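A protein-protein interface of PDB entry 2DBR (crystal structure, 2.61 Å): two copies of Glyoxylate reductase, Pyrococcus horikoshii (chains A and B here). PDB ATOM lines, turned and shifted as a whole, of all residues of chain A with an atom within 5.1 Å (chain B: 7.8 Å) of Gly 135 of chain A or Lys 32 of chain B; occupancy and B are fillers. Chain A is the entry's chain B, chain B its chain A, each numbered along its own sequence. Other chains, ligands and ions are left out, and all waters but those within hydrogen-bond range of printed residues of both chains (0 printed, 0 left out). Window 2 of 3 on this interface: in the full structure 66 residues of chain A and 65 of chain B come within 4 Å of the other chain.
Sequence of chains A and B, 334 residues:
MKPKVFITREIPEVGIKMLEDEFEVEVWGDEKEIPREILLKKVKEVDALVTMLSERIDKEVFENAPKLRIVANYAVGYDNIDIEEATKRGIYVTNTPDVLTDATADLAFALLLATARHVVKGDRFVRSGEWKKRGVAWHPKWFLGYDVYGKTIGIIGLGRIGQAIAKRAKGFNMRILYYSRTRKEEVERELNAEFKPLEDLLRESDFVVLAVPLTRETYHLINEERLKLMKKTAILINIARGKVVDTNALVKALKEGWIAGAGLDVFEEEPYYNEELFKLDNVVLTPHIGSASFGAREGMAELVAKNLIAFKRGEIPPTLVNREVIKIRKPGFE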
ATOM      1  N   TRP A 131     -16.379  18.232   2.104  1.00  0.00           N
ATOM      2  CA  TRP A 131     -17.199  19.349   2.542  1.00  0.00           C
ATOM      3  C   TRP A 131     -16.730  20.643   1.883  1.00  0.00           C
ATOM      4  O   TRP A 131     -17.532  21.385   1.319  1.00  0.00           O
ATOM      5  CB  TRP A 131     -17.132  19.467   4.064  1.00  0.00           C
ATOM      6  CG  TRP A 131     -18.011  20.536   4.640  1.00  0.00           C
ATOM      7  CD1 TRP A 131     -19.226  20.946   4.168  1.00  0.00           C
ATOM      8  CD2 TRP A 131     -17.775  21.281   5.842  1.00  0.00           C
ATOM      9  NE1 TRP A 131     -19.764  21.898   5.001  1.00  0.00           N
ATOM     10  CE2 TRP A 131     -18.897  22.124   6.037  1.00  0.00           C
ATOM     11  CE3 TRP A 131     -16.726  21.316   6.774  1.00  0.00           C
ATOM     12  CZ2 TRP A 131     -19.002  22.998   7.132  1.00  0.00           C
ATOM     13  CZ3 TRP A 131     -16.828  22.186   7.864  1.00  0.00           C
ATOM     14  CH2 TRP A 131     -17.962  23.016   8.033  1.00  0.00           C
ATOM     15  N   LYS A 132     -15.432  20.912   1.960  1.00  0.00           N
ATOM     16  CA  LYS A 132     -14.863  22.107   1.353  1.00  0.00           C
ATOM     17  C   LYS A 132     -15.142  22.001  -0.146  1.00  0.00           C
ATOM     18  O   LYS A 132     -15.724  22.902  -0.759  1.00  0.00           O
ATOM     19  CB  LYS A 132     -13.347  22.158   1.617  1.00  0.00           C
ATOM     20  CG  LYS A 132     -12.614  23.386   1.072  1.00  0.00           C
ATOM     21  CD  LYS A 132     -13.045  24.657   1.791  1.00  0.00           C
ATOM     22  CE  LYS A 132     -12.321  25.893   1.254  1.00  0.00           C
ATOM     23  NZ  LYS A 132     -12.675  27.143   2.015  1.00  0.00           N
ATOM     24  N   LYS A 133     -14.742  20.872  -0.717  1.00  0.00           N
ATOM     25  CA  LYS A 133     -14.919  20.596  -2.138  1.00  0.00           C
ATOM     26  C   LYS A 133     -16.319  20.962  -2.643  1.00  0.00           C
ATOM     27  O   LYS A 133     -16.461  21.604  -3.682  1.00  0.00           O
ATOM     28  CB  LYS A 133     -14.625  19.108  -2.408  1.00  0.00           C
ATOM     29  CG  LYS A 133     -14.203  18.785  -3.840  1.00  0.00           C
ATOM     30  CD  LYS A 133     -15.376  18.384  -4.729  1.00  0.00           C
ATOM     31  CE  LYS A 133     -15.780  16.938  -4.497  1.00  0.00           C
ATOM     32  NZ  LYS A 133     -17.036  16.584  -5.224  1.00  0.00           N
ATOM     33  N   ARG A 134     -17.350  20.564  -1.908  1.00  0.00           N
ATOM     34  CA  ARG A 134     -18.711  20.861  -2.327  1.00  0.00           C
ATOM     35  C   ARG A 134     -19.035  22.351  -2.183  1.00  0.00           C
ATOM     36  O   ARG A 134     -19.998  22.854  -2.768  1.00  0.00           O
ATOM     37  CB  ARG A 134     -19.702  20.001  -1.538  1.00  0.00           C
ATOM     38  CG  ARG A 134     -21.111  20.026  -2.102  1.00  0.00           C
ATOM     39  CD  ARG A 134     -21.857  18.758  -1.771  1.00  0.00           C
ATOM     40  NE  ARG A 134     -23.274  18.888  -2.078  1.00  0.00           N
ATOM     41  CZ  ARG A 134     -24.166  17.919  -1.906  1.00  0.00           C
ATOM     42  NH1 ARG A 134     -23.788  16.737  -1.431  1.00  0.00           N
ATOM     43  NH2 ARG A 134     -25.442  18.137  -2.198  1.00  0.00           N
ATOM     44  N   GLY A 135     -18.224  23.056  -1.405  1.00  0.00           N
ATOM     45  CA  GLY A 135     -18.414  24.484  -1.249  1.00  0.00           C
ATOM     46  C   GLY A 135     -19.641  24.999  -0.524  1.00  0.00           C
ATOM     47  O   GLY A 135     -19.900  26.203  -0.537  1.00  0.00           O
ATOM     48  N   VAL A 136     -20.413  24.120   0.098  1.00  0.00           N
ATOM     49  CA  VAL A 136     -21.580  24.581   0.832  1.00  0.00           C
ATOM     50  C   VAL A 136     -21.228  24.507   2.308  1.00  0.00           C
ATOM     51  O   VAL A 136     -20.815  23.462   2.808  1.00  0.00           O
ATOM     52  CB  VAL A 136     -22.816  23.717   0.545  1.00  0.00           C
ATOM     53  CG1 VAL A 136     -24.048  24.372   1.140  1.00  0.00           C
ATOM     54  CG2 VAL A 136     -22.982  23.532  -0.953  1.00  0.00           C
ATOM     55  N   ALA A 137     -21.383  25.621   3.005  1.00  0.00           N
ATOM     56  CA  ALA A 137     -21.043  25.670   4.415  1.00  0.00           C
ATOM     57  C   ALA A 137     -22.049  25.012   5.350  1.00  0.00           C
ATOM     58  O   ALA A 137     -21.699  24.104   6.105  1.00  0.00           O
ATOM     59  CB  ALA A 137     -20.825  27.117   4.837  1.00  0.00           C
ATOM     60  N   THR B   8     -33.380  33.400   2.510  1.00  0.00           N
ATOM     61  CA  THR B   8     -32.116  33.003   1.894  1.00  0.00           C
ATOM     62  C   THR B   8     -31.782  31.518   1.753  1.00  0.00           C
ATOM     63  O   THR B   8     -30.714  31.180   1.246  1.00  0.00           O
ATOM     64  CB  THR B   8     -30.946  33.689   2.604  1.00  0.00           C
ATOM     65  OG1 THR B   8     -31.040  33.457   4.015  1.00  0.00           O
ATOM     66  CG2 THR B   8     -30.973  35.188   2.332  1.00  0.00           C
ATOM     67  N   ARG B   9     -32.668  30.633   2.197  1.00  0.00           N
ATOM     68  CA  ARG B   9     -32.422  29.196   2.071  1.00  0.00           C
ATOM     69  C   ARG B   9     -33.671  28.360   2.316  1.00  0.00           C
ATOM     70  O   ARG B   9     -34.612  28.809   2.966  1.00  0.00           O
ATOM     71  CB  ARG B   9     -31.329  28.736   3.034  1.00  0.00           C
ATOM     72  CG  ARG B   9     -30.739  27.395   2.645  1.00  0.00           C
ATOM     73  CD  ARG B   9     -29.937  27.540   1.366  1.00  0.00           C
ATOM     74  NE  ARG B   9     -28.753  28.351   1.607  1.00  0.00           N
ATOM     75  CZ  ARG B   9     -27.647  27.904   2.191  1.00  0.00           C
ATOM     76  NH1 ARG B   9     -27.560  26.643   2.583  1.00  0.00           N
ATOM     77  NH2 ARG B   9     -26.633  28.727   2.410  1.00  0.00           N
ATOM     78  N   TRP B  28     -34.800  31.189  -1.649  1.00  0.00           N
ATOM     79  CA  TRP B  28     -33.620  30.848  -2.438  1.00  0.00           C
ATOM     80  C   TRP B  28     -33.524  29.337  -2.615  1.00  0.00           C
ATOM     81  O   TRP B  28     -33.256  28.603  -1.667  1.00  0.00           O
ATOM     82  CB  TRP B  28     -32.361  31.393  -1.751  1.00  0.00           C
ATOM     83  CG  TRP B  28     -31.063  31.040  -2.436  1.00  0.00           C
ATOM     84  CD1 TRP B  28     -30.154  30.098  -2.042  1.00  0.00           C
ATOM     85  CD2 TRP B  28     -30.533  31.636  -3.624  1.00  0.00           C
ATOM     86  NE1 TRP B  28     -29.090  30.072  -2.911  1.00  0.00           N
ATOM     87  CE2 TRP B  28     -29.297  31.005  -3.891  1.00  0.00           C
ATOM     88  CE3 TRP B  28     -30.982  32.642  -4.488  1.00  0.00           C
ATOM     89  CZ2 TRP B  28     -28.505  31.346  -4.986  1.00  0.00           C
ATOM     90  CZ3 TRP B  28     -30.198  32.981  -5.575  1.00  0.00           C
ATOM     91  CH2 TRP B  28     -28.969  32.335  -5.816  1.00  0.00           C
ATOM     92  N   GLY B  29     -33.738  28.885  -3.845  1.00  0.00           N
ATOM     93  CA  GLY B  29     -33.710  27.466  -4.136  1.00  0.00           C
ATOM     94  C   GLY B  29     -32.388  26.726  -4.095  1.00  0.00           C
ATOM     95  O   GLY B  29     -32.305  25.664  -3.483  1.00  0.00           O
ATOM     96  N   ASP B  30     -31.357  27.261  -4.741  1.00  0.00           N
ATOM     97  CA  ASP B  30     -30.059  26.593  -4.776  1.00  0.00           C
ATOM     98  C   ASP B  30     -29.577  26.126  -3.401  1.00  0.00           C
ATOM     99  O   ASP B  30     -29.840  26.773  -2.386  1.00  0.00           O
ATOM    100  CB  ASP B  30     -29.015  27.514  -5.411  1.00  0.00           C
ATOM    101  CG  ASP B  30     -27.711  26.795  -5.710  1.00  0.00           C
ATOM    102  OD1 ASP B  30     -26.978  26.456  -4.754  1.00  0.00           O
ATOM    103  OD2 ASP B  30     -27.425  26.557  -6.903  1.00  0.00           O
ATOM    104  N   GLU B  31     -28.869  24.997  -3.373  1.00  0.00           N
ATOM    105  CA  GLU B  31     -28.364  24.454  -2.117  1.00  0.00           C
ATOM    106  C   GLU B  31     -27.213  25.278  -1.540  1.00  0.00           C
ATOM    107  O   GLU B  31     -27.184  25.553  -0.338  1.00  0.00           O
ATOM    108  CB  GLU B  31     -27.904  23.003  -2.299  1.00  0.00           C
ATOM    109  CG  GLU B  31     -26.619  22.829  -3.094  1.00  0.00           C
ATOM    110  CD  GLU B  31     -25.995  21.450  -2.909  1.00  0.00           C
ATOM    111  OE1 GLU B  31     -24.907  21.199  -3.471  1.00  0.00           O
ATOM    112  OE2 GLU B  31     -26.592  20.616  -2.196  1.00  0.00           O
ATOM    113  N   LYS B  32     -26.265  25.666  -2.393  1.00  0.00           N
ATOM    114  CA  LYS B  32     -25.113  26.453  -1.951  1.00  0.00           C
ATOM    115  C   LYS B  32     -25.539  27.882  -1.638  1.00  0.00           C
ATOM    116  O   LYS B  32     -26.349  28.461  -2.362  1.00  0.00           O
ATOM    117  CB  LYS B  32     -24.024  26.463  -3.032  1.00  0.00           C
ATOM    118  CG  LYS B  32     -22.687  27.049  -2.573  1.00  0.00           C
ATOM    119  CD  LYS B  32     -21.656  27.075  -3.706  1.00  0.00           C
ATOM    120  CE  LYS B  32     -21.299  25.671  -4.191  1.00  0.00           C
ATOM    121  NZ  LYS B  32     -20.360  25.684  -5.352  1.00  0.00           N
ATOM    122  N   GLU B  33     -24.991  28.438  -0.557  1.00  0.00           N
ATOM    123  CA  GLU B  33     -25.305  29.800  -0.120  1.00  0.00           C
ATOM    124  C   GLU B  33     -25.619  30.751  -1.286  1.00  0.00           C
ATOM    125  O   GLU B  33     -25.167  30.541  -2.411  1.00  0.00           O
ATOM    126  CB  GLU B  33     -24.139  30.382   0.694  1.00  0.00           C
ATOM    127  CG  GLU B  33     -23.892  29.776   2.083  1.00  0.00           C
ATOM    128  CD  GLU B  33     -23.448  28.319   2.049  1.00  0.00           C
ATOM    129  OE1 GLU B  33     -22.789  27.918   1.065  1.00  0.00           O
ATOM    130  OE2 GLU B  33     -23.742  27.578   3.015  1.00  0.00           O
ATOM    131  N   ILE B  34     -26.394  31.797  -1.007  1.00  0.00           N
ATOM    132  CA  ILE B  34     -26.746  32.779  -2.033  1.00  0.00           C
ATOM    133  C   ILE B  34     -25.558  33.707  -2.314  1.00  0.00           C
ATOM    134  O   ILE B  34     -24.941  34.245  -1.392  1.00  0.00           O
ATOM    135  CB  ILE B  34     -27.956  33.646  -1.603  1.00  0.00           C
ATOM    136  CG1 ILE B  34     -28.337  34.599  -2.738  1.00  0.00           C
ATOM    137  CG2 ILE B  34     -27.619  34.444  -0.349  1.00  0.00           C
ATOM    138  CD1 ILE B  34     -29.451  35.562  -2.389  1.00  0.00           C
ATOM    139  N   PRO B  35     -25.221  33.902  -3.601  1.00  0.00           N
ATOM    140  CA  PRO B  35     -24.101  34.772  -3.972  1.00  0.00           C
ATOM    141  C   PRO B  35     -24.274  36.169  -3.401  1.00  0.00           C
ATOM    142  O   PRO B  35     -25.366  36.733  -3.455  1.00  0.00           O
ATOM    143  CB  PRO B  35     -24.151  34.756  -5.494  1.00  0.00           C
ATOM    144  CG  PRO B  35     -24.684  33.385  -5.789  1.00  0.00           C
ATOM    145  CD  PRO B  35     -25.806  33.268  -4.795  1.00  0.00           C
ATOM    146  N   SER B  54     -24.893  32.121   7.454  1.00  0.00           N
ATOM    147  CA  SER B  54     -23.955  32.220   6.343  1.00  0.00           C
ATOM    148  C   SER B  54     -23.970  33.596   5.689  1.00  0.00           C
ATOM    149  O   SER B  54     -22.945  34.061   5.191  1.00  0.00           O
ATOM    150  CB  SER B  54     -24.278  31.166   5.282  1.00  0.00           C
ATOM    151  OG  SER B  54     -23.971  29.861   5.743  1.00  0.00           O
ATOM    152  N   GLU B  55     -25.132  34.240   5.667  1.00  0.00           N
ATOM    153  CA  GLU B  55     -25.224  35.559   5.063  1.00  0.00           C
ATOM    154  C   GLU B  55     -24.607  36.603   5.979  1.00  0.00           C
ATOM    155  O   GLU B  55     -24.800  36.570   7.194  1.00  0.00           O
ATOM    156  CB  GLU B  55     -26.680  35.934   4.773  1.00  0.00           C
ATOM    157  CG  GLU B  55     -27.291  35.250   3.564  1.00  0.00           C
ATOM    158  CD  GLU B  55     -27.591  33.784   3.804  1.00  0.00           C
ATOM    159  OE1 GLU B  55     -28.441  33.483   4.674  1.00  0.00           O
ATOM    160  OE2 GLU B  55     -26.978  32.936   3.122  1.00  0.00           O
ATOM    161  N   GLU B 270     -15.836  28.286   7.051  1.00  0.00           N
ATOM    162  CA  GLU B 270     -16.755  27.236   6.623  1.00  0.00           C
ATOM    163  C   GLU B 270     -17.269  27.400   5.189  1.00  0.00           C
ATOM    164  O   GLU B 270     -17.723  28.476   4.813  1.00  0.00           O
ATOM    165  CB  GLU B 270     -17.933  27.168   7.606  1.00  0.00           C
ATOM    166  CG  GLU B 270     -17.585  26.459   8.914  1.00  0.00           C
ATOM    167  CD  GLU B 270     -18.515  26.813  10.052  1.00  0.00           C
ATOM    168  OE1 GLU B 270     -19.650  27.251   9.774  1.00  0.00           O
ATOM    169  OE2 GLU B 270     -18.117  26.645  11.225  1.00  0.00           O
ATOM    170  N   PRO B 271     -17.205  26.329   4.371  1.00  0.00           N
ATOM    171  CA  PRO B 271     -16.684  24.999   4.721  1.00  0.00           C
ATOM    172  C   PRO B 271     -15.219  25.073   5.132  1.00  0.00           C
ATOM    173  O   PRO B 271     -14.577  26.094   4.938  1.00  0.00           O
ATOM    174  CB  PRO B 271     -16.912  24.182   3.447  1.00  0.00           C
ATOM    175  CG  PRO B 271     -16.926  25.217   2.365  1.00  0.00           C
ATOM    176  CD  PRO B 271     -17.710  26.338   2.989  1.00  0.00           C
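OE2 of Glu 31 of chain B lies within salt-bridge range of NH2 of Arg 134 of chain A (2.7 Å). The side-chain carboxylate of Glu 33 of chain B is in hydrogen-bond range of the backbone NH of Ala 137 of chain A, at 3.1 Å.
NE1 of Trp 28 of chain B is in hydrogen-bond range of O of Lys 32 of chain B, 3.2 Å away. NH1 of Arg 9 of chain B is in hydrogen-bond range of O of Glu 31 of chain B (3.1 Å). OD1 of Asp 30 of chain B sits at hydrogen-bond distance from N of Lys 32 of chain B. The indole nitrogen of Trp 131 of chain A sits close to the backbone carbonyl oxygen of Ala 137 of chain A. OE2 of Glu 33 of chain B is in salt-bridge range of NH2 of Arg 9 of chain B (3.2 Å). The backbone carbonyl oxygen of Val 136 of chain A lies within hydrogen-bond range of the indole nitrogen of Trp 131 of chain A, at 2.9 Å.
Among the printed residues, merely in contact across the chains: Ala 137 of chain A with Glu 270 of chain B (3.4 Å), Arg 134 of chain A with Lys 32 of chain B (3.4 Å), Gly 135 of chain A with Lys 32 of chain B (3.6 Å), Val 136 of chain A with Glu 33 of chain B (3.6 Å), Trp 131 of chain A with Pro 271 of chain B (3.6 Å), Trp 131 of chain A with Glu 270 of chain B (3.6 Å), Lys 132 of chain A with Pro 271 of chain B (3.6 Å), Val 136 of chain A with Glu 31 of chain B (3.7 Å), Ala 137 of chain A with Pro 271 of chain B (3.7 Å), Gly 135 of chain A with Glu 33 of chain B (3.7 Å), Val 136 of chain A with Lys 32 of chain B (3.7 Å) and Gly 135 of chain A with Pro 271 of chain B (3.97 Å).
Printed residues of chain B within 4 Å of Gly 135 of chain A: Lys 32, Glu 33 and Pro 271. Of the printed residues of chain A, Lys 32 of chain B touches Arg 134, Gly 135 and Val 136. Printed residues of chain B within 4 Å of Val 136 of chain A: Glu 31 (3.7 Å), Lys 32 (3.7 Å) and Glu 33 (3.6 Å). Of the printed residues of chain B, Trp 131 of chain A touches Glu 270 (3.6 Å) and Pro 271 (3.6 Å). The nearest residue of chain B that does not touch Gly 135 of chain A is Glu 270 of chain B (6.2 Å). The nearest printed residue of chain A that does not touch Lys 32 of chain B is Lys 133 of chain A (5.9 Å).
Printed residues of chain B that touch a printed residue of chain A: Glu 31, Lys 32, Glu 33, Glu 270 and Pro 271. Of the 7 printed residues of chain A, 6 touch a printed residue of chain B. Among the printed residues, 14 pairs touch across the chains. Among the printed residues, Asp or Glu carboxylates within 4 Å of a Lys or Arg side-chain nitrogen of the other chain: Arg 134 of chain A with Glu 31 of chain B.
No position is printed for both chains.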
